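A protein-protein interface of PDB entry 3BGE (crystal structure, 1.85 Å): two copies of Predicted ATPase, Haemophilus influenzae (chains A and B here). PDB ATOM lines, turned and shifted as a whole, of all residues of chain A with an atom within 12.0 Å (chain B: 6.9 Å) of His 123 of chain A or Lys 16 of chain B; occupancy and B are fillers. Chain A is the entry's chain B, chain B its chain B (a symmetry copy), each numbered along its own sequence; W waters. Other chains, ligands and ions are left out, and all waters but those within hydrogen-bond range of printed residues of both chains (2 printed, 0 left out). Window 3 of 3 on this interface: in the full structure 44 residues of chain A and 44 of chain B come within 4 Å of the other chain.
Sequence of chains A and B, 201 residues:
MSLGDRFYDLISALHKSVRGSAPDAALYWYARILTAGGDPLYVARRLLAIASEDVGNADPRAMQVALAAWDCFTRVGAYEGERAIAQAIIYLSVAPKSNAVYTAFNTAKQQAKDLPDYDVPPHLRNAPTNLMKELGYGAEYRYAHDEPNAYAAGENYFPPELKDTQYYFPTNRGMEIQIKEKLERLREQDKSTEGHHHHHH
The side-chain hydroxyl of Ser 17 of chain B is in hydrogen-bond range of the backbone carbonyl oxygen of Ala 13 of chain B, at 2.8 Å. The backbone carbonyl oxygen (O) of Ser 17 of chain B is in hydrogen-bond range of the backbone NH (N) of Ala 22 of chain B, 2.8 Å away. The guanidinium group (NH2) of Arg 125 of chain A sits at hydrogen-bond distance from the backbone carbonyl oxygen (O) of Val 120 of chain A, 2.8 Å away.
Water W2 lies within hydrogen-bond range of O of Lys 16 of chain B, OH of Tyr 157 of chain A and N of Gly 20 of chain B. Water W1 bridges the guanidinium group (NH1) of Arg 19 of chain B and the backbone carbonyl oxygen (O) of Pro 128 of chain A.
No position is printed for both chains.
OG of Ser 12 of chain B lies within hydrogen-bond range of N of Asn 126 of chain A. ND1 of His 15 of chain B is in hydrogen-bond range of O of Ala 127 of chain A (2.8 Å). The side-chain amino group of Lys 16 of chain B sits at hydrogen-bond distance from the backbone carbonyl oxygen of His 123 of chain A (2.6 Å). The backbone carbonyl oxygen (O) of Leu 124 of chain A is in hydrogen-bond range of the backbone NH (N) of Ala 13 of chain B (3.5 Å). The backbone carbonyl oxygen (O) of Leu 124 of chain A is in hydrogen-bond range of the side-chain hydroxyl (OG) of Ser 12 of chain B. The backbone NH of Ala 127 of chain A is in hydrogen-bond range of the side-chain hydroxyl of Ser 12 of chain B (2.6 Å).
Of the printed residues of chain B, Arg 125 of chain A touches Ser 12 (3.2 Å) and Lys 16 (3.8 Å). Leu 162 of chain A touches none of the printed residues of chain B. Asp 164 of chain A touches none of the printed residues of chain B. Of the printed residues of chain A, Leu 10 of chain B touches Val 120. Leu 14 of chain B touches none of the printed residues of chain A. Of chain A, only Ala 127, Pro 128 and Thr 129 come within 4 Å of His 15 of chain B. Of chain A, only His 123 (2.6 Å), Leu 124 (3.9 Å), Arg 125 (3.8 Å), Ala 127 (3.7 Å) and Tyr 157 (3.3 Å) come within 4 Å of Lys 16 of chain B. Printed residues of chain A within 4 Å of Ser 17 of chain B: Tyr 157. No residue of chain A comes within 4 Å of Val 18 of chain B. Arg 19 of chain B touches one residue of chain A. No residue of chain A comes within 4 Å of Ser 21 of chain B. Ala 22 of chain B touches just one residue of chain A: Tyr 157 (3.5 Å). The nearest printed residue of chain B that does not touch His 123 of chain A is Ser 12 of chain B (6.6 Å).
Hydrophobic or aromatic side chains of chain A within 4 Å of the printed part of chain B: Val 120, Leu 124, Ala 127 and Tyr 157. Of the 14 printed residues of chain B, 9 touch a printed residue of chain A. Among the printed residues, 19 pairs touch across the chains. Among the printed residues, no Asp or Glu carboxylate lies within 4 Å of a Lys or Arg side-chain nitrogen of the other chain.
Among the printed residues, pairs that only touch across the chains: Arg 125 of chain A with Ser 12 of chain B, Tyr 157 of chain A with Lys 16 of chain B, Tyr 157 of chain A with Gly 20 of chain B, Tyr 157 of chain A with Ala 22 of chain B, Pro 128 of chain A with His 15 of chain B, Tyr 157 of chain A with Ser 17 of chain B, Val 120 of chain A with Leu 10 of chain B, Ala 127 of chain A with Lys 16 of chain B, Ala 127 of chain A with Arg 19 of chain B, Arg 125 of chain A with Lys 16 of chain B, Val 120 of chain A with Ala 13 of chain B, Thr 129 of chain A with His 15 of chain B and Leu 124 of chain A with Lys 16 of chain B.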
ATOM      1  N   TYR A 118      15.203 -13.464  32.492  1.00  0.00           N
ATOM      2  CA  TYR A 118      14.968 -12.472  33.543  1.00  0.00           C
ATOM      3  C   TYR A 118      13.508 -12.090  33.745  1.00  0.00           C
ATOM      4  O   TYR A 118      12.743 -11.943  32.771  1.00  0.00           O
ATOM      5  CB  TYR A 118      15.758 -11.176  33.277  1.00  0.00           C
ATOM      6  CG  TYR A 118      17.234 -11.364  33.094  1.00  0.00           C
ATOM      7  CD1 TYR A 118      18.012 -11.879  34.119  1.00  0.00           C
ATOM      8  CD2 TYR A 118      17.867 -10.991  31.896  1.00  0.00           C
ATOM      9  CE1 TYR A 118      19.372 -12.061  33.967  1.00  0.00           C
ATOM     10  CE2 TYR A 118      19.229 -11.169  31.724  1.00  0.00           C
ATOM     11  CZ  TYR A 118      19.985 -11.703  32.784  1.00  0.00           C
ATOM     12  OH  TYR A 118      21.361 -11.893  32.673  1.00  0.00           O
ATOM     13  N   ASP A 119      13.131 -11.900  35.015  1.00  0.00           N
ATOM     14  CA  ASP A 119      11.788 -11.458  35.341  1.00  0.00           C
ATOM     15  C   ASP A 119      11.479 -10.115  34.691  1.00  0.00           C
ATOM     16  O   ASP A 119      12.387  -9.298  34.423  1.00  0.00           O
ATOM     17  CB  ASP A 119      11.584 -11.302  36.852  1.00  0.00           C
ATOM     18  CG  ASP A 119      11.689 -12.612  37.593  1.00  0.00           C
ATOM     19  OD1 ASP A 119      11.662 -13.686  36.933  1.00  0.00           O
ATOM     20  OD2 ASP A 119      11.794 -12.561  38.840  1.00  0.00           O
ATOM     21  N   VAL A 120      10.184  -9.865  34.479  1.00  0.00           N
ATOM     22  CA  VAL A 120       9.769  -8.503  34.104  1.00  0.00           C
ATOM     23  C   VAL A 120       9.911  -7.579  35.329  1.00  0.00           C
ATOM     24  O   VAL A 120       9.313  -7.842  36.383  1.00  0.00           O
ATOM     25  CB  VAL A 120       8.298  -8.454  33.566  1.00  0.00           C
ATOM     26  CG1 VAL A 120       7.856  -7.001  33.307  1.00  0.00           C
ATOM     27  CG2 VAL A 120       8.149  -9.369  32.326  1.00  0.00           C
ATOM     28  N   PRO A 121      10.688  -6.487  35.183  1.00  0.00           N
ATOM     29  CA  PRO A 121      10.869  -5.573  36.325  1.00  0.00           C
ATOM     30  C   PRO A 121       9.492  -5.130  36.846  1.00  0.00           C
ATOM     31  O   PRO A 121       8.614  -4.769  36.041  1.00  0.00           O
ATOM     32  CB  PRO A 121      11.649  -4.401  35.720  1.00  0.00           C
ATOM     33  CG  PRO A 121      12.357  -4.976  34.495  1.00  0.00           C
ATOM     34  CD  PRO A 121      11.388  -6.042  33.970  1.00  0.00           C
ATOM     35  N   PRO A 122       9.276  -5.162  38.179  1.00  0.00           N
ATOM     36  CA  PRO A 122       7.913  -4.862  38.629  1.00  0.00           C
ATOM     37  C   PRO A 122       7.286  -3.575  38.090  1.00  0.00           C
ATOM     38  O   PRO A 122       6.084  -3.562  37.808  1.00  0.00           O
ATOM     39  CB  PRO A 122       8.051  -4.851  40.155  1.00  0.00           C
ATOM     40  CG  PRO A 122       9.139  -5.855  40.405  1.00  0.00           C
ATOM     41  CD  PRO A 122      10.152  -5.496  39.325  1.00  0.00           C
ATOM     42  N   HIS A 123       8.072  -2.517  37.910  1.00  0.00           N
ATOM     43  CA  HIS A 123       7.520  -1.256  37.421  1.00  0.00           C
ATOM     44  C   HIS A 123       7.102  -1.286  35.950  1.00  0.00           C
ATOM     45  O   HIS A 123       6.527  -0.323  35.460  1.00  0.00           O
ATOM     46  CB  HIS A 123       8.487  -0.099  37.668  1.00  0.00           C
ATOM     47  CG  HIS A 123       9.788  -0.239  36.942  1.00  0.00           C
ATOM     48  ND1 HIS A 123      10.849  -0.962  37.450  1.00  0.00           N
ATOM     49  CD2 HIS A 123      10.196   0.235  35.741  1.00  0.00           C
ATOM     50  CE1 HIS A 123      11.859  -0.913  36.598  1.00  0.00           C
ATOM     51  NE2 HIS A 123      11.487  -0.195  35.551  1.00  0.00           N
ATOM     52  N   LEU A 124       7.382  -2.384  35.246  1.00  0.00           N
ATOM     53  CA  LEU A 124       6.950  -2.520  33.844  1.00  0.00           C
ATOM     54  C   LEU A 124       5.693  -3.365  33.715  1.00  0.00           C
ATOM     55  O   LEU A 124       5.147  -3.514  32.632  1.00  0.00           O
ATOM     56  CB  LEU A 124       8.069  -3.092  32.962  1.00  0.00           C
ATOM     57  CG  LEU A 124       9.330  -2.226  32.886  1.00  0.00           C
ATOM     58  CD1 LEU A 124      10.359  -2.857  31.957  1.00  0.00           C
ATOM     59  CD2 LEU A 124       8.988  -0.846  32.406  1.00  0.00           C
ATOM     60  N   ARG A 125       5.237  -3.911  34.836  1.00  0.00           N
ATOM     61  CA  ARG A 125       4.023  -4.727  34.861  1.00  0.00           C
ATOM     62  C   ARG A 125       2.717  -3.912  34.868  1.00  0.00           C
ATOM     63  O   ARG A 125       2.712  -2.690  35.077  1.00  0.00           O
ATOM     64  CB  ARG A 125       4.078  -5.686  36.039  1.00  0.00           C
ATOM     65  CG  ARG A 125       5.332  -6.522  36.006  1.00  0.00           C
ATOM     66  CD  ARG A 125       5.357  -7.532  37.109  1.00  0.00           C
ATOM     67  NE  ARG A 125       6.668  -8.145  37.254  1.00  0.00           N
ATOM     68  CZ  ARG A 125       6.955  -9.070  38.172  1.00  0.00           C
ATOM     69  NH1 ARG A 125       6.009  -9.472  39.025  1.00  0.00           N
ATOM     70  NH2 ARG A 125       8.173  -9.595  38.240  1.00  0.00           N
ATOM     71  N   ASN A 126       1.607  -4.595  34.617  1.00  0.00           N
ATOM     72  CA  ASN A 126       0.304  -3.921  34.528  1.00  0.00           C
ATOM     73  C   ASN A 126       0.280  -2.686  33.601  1.00  0.00           C
ATOM     74  O   ASN A 126       0.194  -1.537  34.064  1.00  0.00           O
ATOM     75  CB  ASN A 126      -0.205  -3.575  35.937  1.00  0.00           C
ATOM     76  CG  ASN A 126      -0.158  -4.774  36.879  1.00  0.00           C
ATOM     77  OD1 ASN A 126      -0.388  -5.913  36.462  1.00  0.00           O
ATOM     78  ND2 ASN A 126       0.158  -4.525  38.146  1.00  0.00           N
ATOM     79  N   ALA A 127       0.399  -2.932  32.295  1.00  0.00           N
ATOM     80  CA  ALA A 127       0.130  -1.916  31.281  1.00  0.00           C
ATOM     81  C   ALA A 127      -0.680  -2.595  30.203  1.00  0.00           C
ATOM     82  O   ALA A 127      -0.168  -2.894  29.126  1.00  0.00           O
ATOM     83  CB  ALA A 127       1.402  -1.315  30.712  1.00  0.00           C
ATOM     84  N   PRO A 128      -1.968  -2.831  30.500  1.00  0.00           N
ATOM     85  CA  PRO A 128      -2.867  -3.606  29.663  1.00  0.00           C
ATOM     86  C   PRO A 128      -3.403  -2.781  28.501  1.00  0.00           C
ATOM     87  O   PRO A 128      -3.137  -1.577  28.415  1.00  0.00           O
ATOM     88  CB  PRO A 128      -4.017  -3.939  30.625  1.00  0.00           C
ATOM     89  CG  PRO A 128      -4.094  -2.721  31.525  1.00  0.00           C
ATOM     90  CD  PRO A 128      -2.645  -2.303  31.707  1.00  0.00           C
ATOM     91  N   THR A 129      -4.173  -3.438  27.630  1.00  0.00           N
ATOM     92  CA  THR A 129      -4.874  -2.773  26.543  1.00  0.00           C
ATOM     93  C   THR A 129      -6.346  -3.197  26.493  1.00  0.00           C
ATOM     94  O   THR A 129      -6.780  -4.091  27.230  1.00  0.00           O
ATOM     95  CB  THR A 129      -4.192  -3.053  25.199  1.00  0.00           C
ATOM     96  OG1 THR A 129      -3.959  -4.460  25.072  1.00  0.00           O
ATOM     97  CG2 THR A 129      -2.860  -2.326  25.112  1.00  0.00           C
ATOM     98  N   ASN A 156      15.086   2.921  32.541  1.00  0.00           N
ATOM     99  CA  ASN A 156      15.469   1.622  31.989  1.00  0.00           C
ATOM    100  C   ASN A 156      14.263   0.710  31.751  1.00  0.00           C
ATOM    101  O   ASN A 156      13.465   0.444  32.650  1.00  0.00           O
ATOM    102  CB  ASN A 156      16.555   0.916  32.848  1.00  0.00           C
ATOM    103  CG  ASN A 156      17.142  -0.353  32.158  1.00  0.00           C
ATOM    104  OD1 ASN A 156      17.213  -0.421  30.911  1.00  0.00           O
ATOM    105  ND2 ASN A 156      17.563  -1.361  32.979  1.00  0.00           N
ATOM    106  N   TYR A 157      14.149   0.247  30.513  1.00  0.00           N
ATOM    107  CA  TYR A 157      13.085  -0.660  30.094  1.00  0.00           C
ATOM    108  C   TYR A 157      13.599  -2.109  29.923  1.00  0.00           C
ATOM    109  O   TYR A 157      12.825  -3.037  29.642  1.00  0.00           O
ATOM    110  CB  TYR A 157      12.453  -0.136  28.810  1.00  0.00           C
ATOM    111  CG  TYR A 157      11.626   1.116  29.023  1.00  0.00           C
ATOM    112  CD1 TYR A 157      10.334   1.033  29.543  1.00  0.00           C
ATOM    113  CD2 TYR A 157      12.140   2.374  28.734  1.00  0.00           C
ATOM    114  CE1 TYR A 157       9.567   2.170  29.753  1.00  0.00           C
ATOM    115  CE2 TYR A 157      11.369   3.526  28.931  1.00  0.00           C
ATOM    116  CZ  TYR A 157      10.089   3.403  29.452  1.00  0.00           C
ATOM    117  OH  TYR A 157       9.304   4.504  29.667  1.00  0.00           O
ATOM    118  N   PHE A 158      14.893  -2.315  30.128  1.00  0.00           N
ATOM    119  CA  PHE A 158      15.445  -3.677  30.088  1.00  0.00           C
ATOM    120  C   PHE A 158      15.502  -4.244  31.505  1.00  0.00           C
ATOM    121  O   PHE A 158      15.474  -3.493  32.487  1.00  0.00           O
ATOM    122  CB  PHE A 158      16.885  -3.685  29.529  1.00  0.00           C
ATOM    123  CG  PHE A 158      16.984  -3.718  28.024  1.00  0.00           C
ATOM    124  CD1 PHE A 158      17.073  -4.927  27.362  1.00  0.00           C
ATOM    125  CD2 PHE A 158      17.070  -2.533  27.289  1.00  0.00           C
ATOM    126  CE1 PHE A 158      17.196  -4.973  25.998  1.00  0.00           C
ATOM    127  CE2 PHE A 158      17.197  -2.567  25.909  1.00  0.00           C
ATOM    128  CZ  PHE A 158      17.263  -3.813  25.268  1.00  0.00           C
ATOM    129  N   PRO A 159      15.627  -5.571  31.625  1.00  0.00           N
ATOM    130  CA  PRO A 159      16.055  -6.049  32.933  1.00  0.00           C
ATOM    131  C   PRO A 159      17.350  -5.307  33.319  1.00  0.00           C
ATOM    132  O   PRO A 159      18.127  -4.900  32.454  1.00  0.00           O
ATOM    133  CB  PRO A 159      16.365  -7.528  32.687  1.00  0.00           C
ATOM    134  CG  PRO A 159      15.525  -7.915  31.458  1.00  0.00           C
ATOM    135  CD  PRO A 159      15.433  -6.653  30.634  1.00  0.00           C
ATOM    136  N   PRO A 160      17.600  -5.171  34.616  1.00  0.00           N
ATOM    137  CA  PRO A 160      18.806  -4.493  35.136  1.00  0.00           C
ATOM    138  C   PRO A 160      20.136  -4.999  34.513  1.00  0.00           C
ATOM    139  O   PRO A 160      21.026  -4.200  34.180  1.00  0.00           O
ATOM    140  CB  PRO A 160      18.781  -4.861  36.615  1.00  0.00           C
ATOM    141  CG  PRO A 160      17.374  -5.110  36.937  1.00  0.00           C
ATOM    142  CD  PRO A 160      16.755  -5.716  35.689  1.00  0.00           C
ATOM    143  N   GLU A 161      20.267  -6.316  34.381  1.00  0.00           N
ATOM    144  CA  GLU A 161      21.444  -6.940  33.792  1.00  0.00           C
ATOM    145  C   GLU A 161      21.696  -6.435  32.379  1.00  0.00           C
ATOM    146  O   GLU A 161      22.847  -6.395  31.932  1.00  0.00           O
ATOM    147  CB  GLU A 161      21.298  -8.477  33.762  1.00  0.00           C
ATOM    148  CG  GLU A 161      21.354  -9.143  35.152  1.00  0.00           C
ATOM    149  CD  GLU A 161      20.016  -9.175  35.908  1.00  0.00           C
ATOM    150  OE1 GLU A 161      19.025  -8.540  35.469  1.00  0.00           O
ATOM    151  OE2 GLU A 161      19.954  -9.851  36.962  1.00  0.00           O
ATOM    152  N   LEU A 162      20.635  -6.010  31.691  1.00  0.00           N
ATOM    153  CA  LEU A 162      20.736  -5.630  30.280  1.00  0.00           C
ATOM    154  C   LEU A 162      20.619  -4.127  30.036  1.00  0.00           C
ATOM    155  O   LEU A 162      20.508  -3.674  28.900  1.00  0.00           O
ATOM    156  CB  LEU A 162      19.699  -6.416  29.453  1.00  0.00           C
ATOM    157  CG  LEU A 162      19.805  -7.940  29.576  1.00  0.00           C
ATOM    158  CD1 LEU A 162      18.699  -8.591  28.733  1.00  0.00           C
ATOM    159  CD2 LEU A 162      21.207  -8.462  29.180  1.00  0.00           C
ATOM    160  N   LYS A 163      20.715  -3.348  31.107  1.00  0.00           N
ATOM    161  CA  LYS A 163      20.705  -1.899  31.015  1.00  0.00           C
ATOM    162  C   LYS A 163      21.653  -1.445  29.920  1.00  0.00           C
ATOM    163  O   LYS A 163      22.790  -1.925  29.840  1.00  0.00           O
ATOM    164  CB  LYS A 163      21.148  -1.274  32.358  1.00  0.00           C
ATOM    165  CG  LYS A 163      20.875   0.220  32.455  1.00  0.00           C
ATOM    166  CD  LYS A 163      21.360   0.816  33.768  1.00  0.00           C
ATOM    167  CE  LYS A 163      21.066   2.304  33.801  1.00  0.00           C
ATOM    168  NZ  LYS A 163      21.991   3.014  34.725  1.00  0.00           N
ATOM    169  N   ASP A 164      21.182  -0.496  29.106  1.00  0.00           N
ATOM    170  CA  ASP A 164      21.963   0.177  28.044  1.00  0.00           C
ATOM    171  C   ASP A 164      22.115  -0.625  26.748  1.00  0.00           C
ATOM    172  O   ASP A 164      22.773  -0.180  25.805  1.00  0.00           O
ATOM    173  CB  ASP A 164      23.344   0.628  28.559  1.00  0.00           C
ATOM    174  CG  ASP A 164      23.241   1.793  29.523  1.00  0.00           C
ATOM    175  OD1 ASP A 164      22.366   2.661  29.311  1.00  0.00           O
ATOM    176  OD2 ASP A 164      24.013   1.829  30.496  1.00  0.00           O
ATOM    177  N   LEU A 183      16.309   9.633  18.481  1.00  0.00           N
ATOM    178  CA  LEU A 183      16.856   8.671  19.428  1.00  0.00           C
ATOM    179  C   LEU A 183      18.171   9.154  20.070  1.00  0.00           C
ATOM    180  O   LEU A 183      18.378   8.989  21.270  1.00  0.00           O
ATOM    181  CB  LEU A 183      17.046   7.323  18.750  1.00  0.00           C
ATOM    182  CG  LEU A 183      15.747   6.612  18.390  1.00  0.00           C
ATOM    183  CD1 LEU A 183      16.093   5.351  17.635  1.00  0.00           C
ATOM    184  CD2 LEU A 183      15.012   6.281  19.667  1.00  0.00           C
ATOM    185  N   LEU A 186      17.264  11.941  22.556  1.00  0.00           N
ATOM    186  CA  LEU A 186      16.722  11.477  23.822  1.00  0.00           C
ATOM    187  C   LEU A 186      17.610  10.431  24.500  1.00  0.00           C
ATOM    188  O   LEU A 186      17.283   9.951  25.583  1.00  0.00           O
ATOM    189  CB  LEU A 186      15.258  11.012  23.679  1.00  0.00           C
ATOM    190  CG  LEU A 186      14.870   9.763  22.883  1.00  0.00           C
ATOM    191  CD1 LEU A 186      15.312   8.491  23.604  1.00  0.00           C
ATOM    192  CD2 LEU A 186      13.363   9.733  22.615  1.00  0.00           C
ATOM    193  N   LEU B  10       4.984  -9.761  30.090  1.00  0.00           N
ATOM    194  CA  LEU B  10       5.840  -9.478  28.916  1.00  0.00           C
ATOM    195  C   LEU B  10       5.232  -8.428  28.013  1.00  0.00           C
ATOM    196  O   LEU B  10       5.912  -7.479  27.588  1.00  0.00           O
ATOM    197  CB  LEU B  10       6.143 -10.762  28.124  1.00  0.00           C
ATOM    198  CG  LEU B  10       6.953 -11.829  28.876  1.00  0.00           C
ATOM    199  CD1 LEU B  10       7.082 -13.167  28.096  1.00  0.00           C
ATOM    200  CD2 LEU B  10       8.345 -11.281  29.242  1.00  0.00           C
ATOM    201  N   ILE B  11       3.934  -8.576  27.751  1.00  0.00           N
ATOM    202  CA  ILE B  11       3.234  -7.685  26.835  1.00  0.00           C
ATOM    203  C   ILE B  11       3.164  -6.313  27.466  1.00  0.00           C
ATOM    204  O   ILE B  11       3.363  -5.285  26.777  1.00  0.00           O
ATOM    205  CB  ILE B  11       1.826  -8.259  26.410  1.00  0.00           C
ATOM    206  CG1 ILE B  11       1.332  -7.607  25.119  1.00  0.00           C
ATOM    207  CG2 ILE B  11       0.815  -8.032  27.500  1.00  0.00           C
ATOM    208  CD1 ILE B  11       2.324  -7.565  23.988  1.00  0.00           C
ATOM    209  N   SER B  12       2.953  -6.291  28.795  1.00  0.00           N
ATOM    210  CA  SER B  12       2.940  -5.044  29.544  1.00  0.00           C
ATOM    211  C   SER B  12       4.264  -4.303  29.403  1.00  0.00           C
ATOM    212  O   SER B  12       4.280  -3.102  29.195  1.00  0.00           O
ATOM    213  CB  SER B  12       2.668  -5.306  31.021  1.00  0.00           C
ATOM    214  OG  SER B  12       2.664  -4.084  31.720  1.00  0.00           O
ATOM    215  N   ALA B  13       5.370  -5.042  29.525  1.00  0.00           N
ATOM    216  CA  ALA B  13       6.723  -4.445  29.454  1.00  0.00           C
ATOM    217  C   ALA B  13       6.930  -3.937  28.020  1.00  0.00           C
ATOM    218  O   ALA B  13       7.483  -2.855  27.811  1.00  0.00           O
ATOM    219  CB  ALA B  13       7.755  -5.502  29.802  1.00  0.00           C
ATOM    220  N   LEU B  14       6.440  -4.703  27.037  1.00  0.00           N
ATOM    221  CA  LEU B  14       6.527  -4.269  25.641  1.00  0.00           C
ATOM    222  C   LEU B  14       5.760  -2.960  25.418  1.00  0.00           C
ATOM    223  O   LEU B  14       6.302  -2.005  24.838  1.00  0.00           O
ATOM    224  CB  LEU B  14       6.035  -5.382  24.687  1.00  0.00           C
ATOM    225  CG  LEU B  14       5.804  -5.068  23.188  1.00  0.00           C
ATOM    226  CD1 LEU B  14       6.915  -4.306  22.573  1.00  0.00           C
ATOM    227  CD2 LEU B  14       5.587  -6.368  22.421  1.00  0.00           C
ATOM    228  N   HIS B  15       4.508  -2.924  25.895  1.00  0.00           N
ATOM    229  CA  HIS B  15       3.664  -1.736  25.824  1.00  0.00           C
ATOM    230  C   HIS B  15       4.383  -0.533  26.432  1.00  0.00           C
ATOM    231  O   HIS B  15       4.489   0.504  25.785  1.00  0.00           O
ATOM    232  CB  HIS B  15       2.343  -2.002  26.547  1.00  0.00           C
ATOM    233  CG  HIS B  15       1.343  -0.894  26.444  1.00  0.00           C
ATOM    234  ND1 HIS B  15       0.187  -0.886  27.191  1.00  0.00           N
ATOM    235  CD2 HIS B  15       1.331   0.249  25.714  1.00  0.00           C
ATOM    236  CE1 HIS B  15      -0.519   0.191  26.890  1.00  0.00           C
ATOM    237  NE2 HIS B  15       0.154   0.896  26.000  1.00  0.00           N
ATOM    238  N   LYS B  16       4.885  -0.693  27.668  1.00  0.00           N
ATOM    239  CA  LYS B  16       5.599   0.372  28.353  1.00  0.00           C
ATOM    240  C   LYS B  16       6.800   0.882  27.555  1.00  0.00           C
ATOM    241  O   LYS B  16       7.094   2.088  27.564  1.00  0.00           O
ATOM    242  CB  LYS B  16       6.037  -0.039  29.768  1.00  0.00           C
ATOM    243  CG  LYS B  16       4.884  -0.076  30.744  1.00  0.00           C
ATOM    244  CD  LYS B  16       5.228   0.587  32.072  1.00  0.00           C
ATOM    245  CE  LYS B  16       3.997   0.689  32.979  1.00  0.00           C
ATOM    246  NZ  LYS B  16       4.366   0.677  34.434  1.00  0.00           N
ATOM    247  N   SER B  17       7.521  -0.029  26.901  1.00  0.00           N
ATOM    248  CA  SER B  17       8.709   0.376  26.157  1.00  0.00           C
ATOM    249  C   SER B  17       8.300   1.150  24.934  1.00  0.00           C
ATOM    250  O   SER B  17       8.909   2.168  24.616  1.00  0.00           O
ATOM    251  CB  SER B  17       9.565  -0.827  25.757  1.00  0.00           C
ATOM    252  OG  SER B  17       9.862  -1.646  26.897  1.00  0.00           O
ATOM    253  N   VAL B  18       7.266   0.678  24.241  1.00  0.00           N
ATOM    254  CA  VAL B  18       6.757   1.439  23.092  1.00  0.00           C
ATOM    255  C   VAL B  18       6.258   2.844  23.512  1.00  0.00           C
ATOM    256  O   VAL B  18       6.671   3.886  22.940  1.00  0.00           O
ATOM    257  CB  VAL B  18       5.608   0.735  22.349  1.00  0.00           C
ATOM    258  CG1 VAL B  18       5.145   1.647  21.210  1.00  0.00           C
ATOM    259  CG2 VAL B  18       6.067  -0.647  21.809  1.00  0.00           C
ATOM    260  N   ARG B  19       5.372   2.892  24.499  1.00  0.00           N
ATOM    261  CA  ARG B  19       4.891   4.196  24.975  1.00  0.00           C
ATOM    262  C   ARG B  19       6.024   5.108  25.488  1.00  0.00           C
ATOM    263  O   ARG B  19       5.954   6.351  25.377  1.00  0.00           O
ATOM    264  CB  ARG B  19       3.724   3.993  25.967  1.00  0.00           C
ATOM    265  CG  ARG B  19       3.767   4.828  27.210  1.00  0.00           C
ATOM    266  CD  ARG B  19       2.379   5.055  27.772  1.00  0.00           C
ATOM    267  NE  ARG B  19       1.579   3.841  27.985  1.00  0.00           N
ATOM    268  CZ  ARG B  19       1.530   3.159  29.134  1.00  0.00           C
ATOM    269  NH1 ARG B  19       0.747   2.086  29.245  1.00  0.00           N
ATOM    270  NH2 ARG B  19       2.272   3.532  30.179  1.00  0.00           N
ATOM    271  N   GLY B  20       7.098   4.498  26.000  1.00  0.00           N
ATOM    272  CA  GLY B  20       8.268   5.230  26.449  1.00  0.00           C
ATOM    273  C   GLY B  20       9.304   5.469  25.359  1.00  0.00           C
ATOM    274  O   GLY B  20      10.429   5.861  25.637  1.00  0.00           O
ATOM    275  N   SER B  21       8.939   5.215  24.110  1.00  0.00           N
ATOM    276  CA  SER B  21       9.826   5.456  22.972  1.00  0.00           C
ATOM    277  C   SER B  21      11.176   4.777  23.145  1.00  0.00           C
ATOM    278  O   SER B  21      12.217   5.376  22.884  1.00  0.00           O
ATOM    279  CB  SER B  21      10.023   6.962  22.707  1.00  0.00           C
ATOM    280  OG  SER B  21       8.778   7.655  22.689  1.00  0.00           O
ATOM    281  N   ALA B  22      11.155   3.532  23.600  1.00  0.00           N
ATOM    282  CA  ALA B  22      12.371   2.741  23.801  1.00  0.00           C
ATOM    283  C   ALA B  22      12.403   1.531  22.862  1.00  0.00           C
ATOM    284  O   ALA B  22      12.100   0.411  23.264  1.00  0.00           O
ATOM    285  CB  ALA B  22      12.473   2.306  25.267  1.00  0.00           C
ATOM    286  N   ILE B  50      -2.124  -0.299  20.790  1.00  0.00           N
ATOM    287  CA  ILE B  50      -1.155   0.769  21.109  1.00  0.00           C
ATOM    288  C   ILE B  50      -1.221   1.945  20.116  1.00  0.00           C
ATOM    289  O   ILE B  50      -1.221   3.108  20.511  1.00  0.00           O
ATOM    290  CB  ILE B  50       0.289   0.182  21.272  1.00  0.00           C
ATOM    291  CG1 ILE B  50       0.355  -0.692  22.519  1.00  0.00           C
ATOM    292  CG2 ILE B  50       1.319   1.296  21.363  1.00  0.00           C
ATOM    293  CD1 ILE B  50       1.443  -1.798  22.503  1.00  0.00           C
HETATM  294  O   HOH W   1      -1.723   0.704  30.129  1.00  0.00           O
HETATM  295  O   HOH W   2       6.121   3.710  29.263  1.00  0.00           O
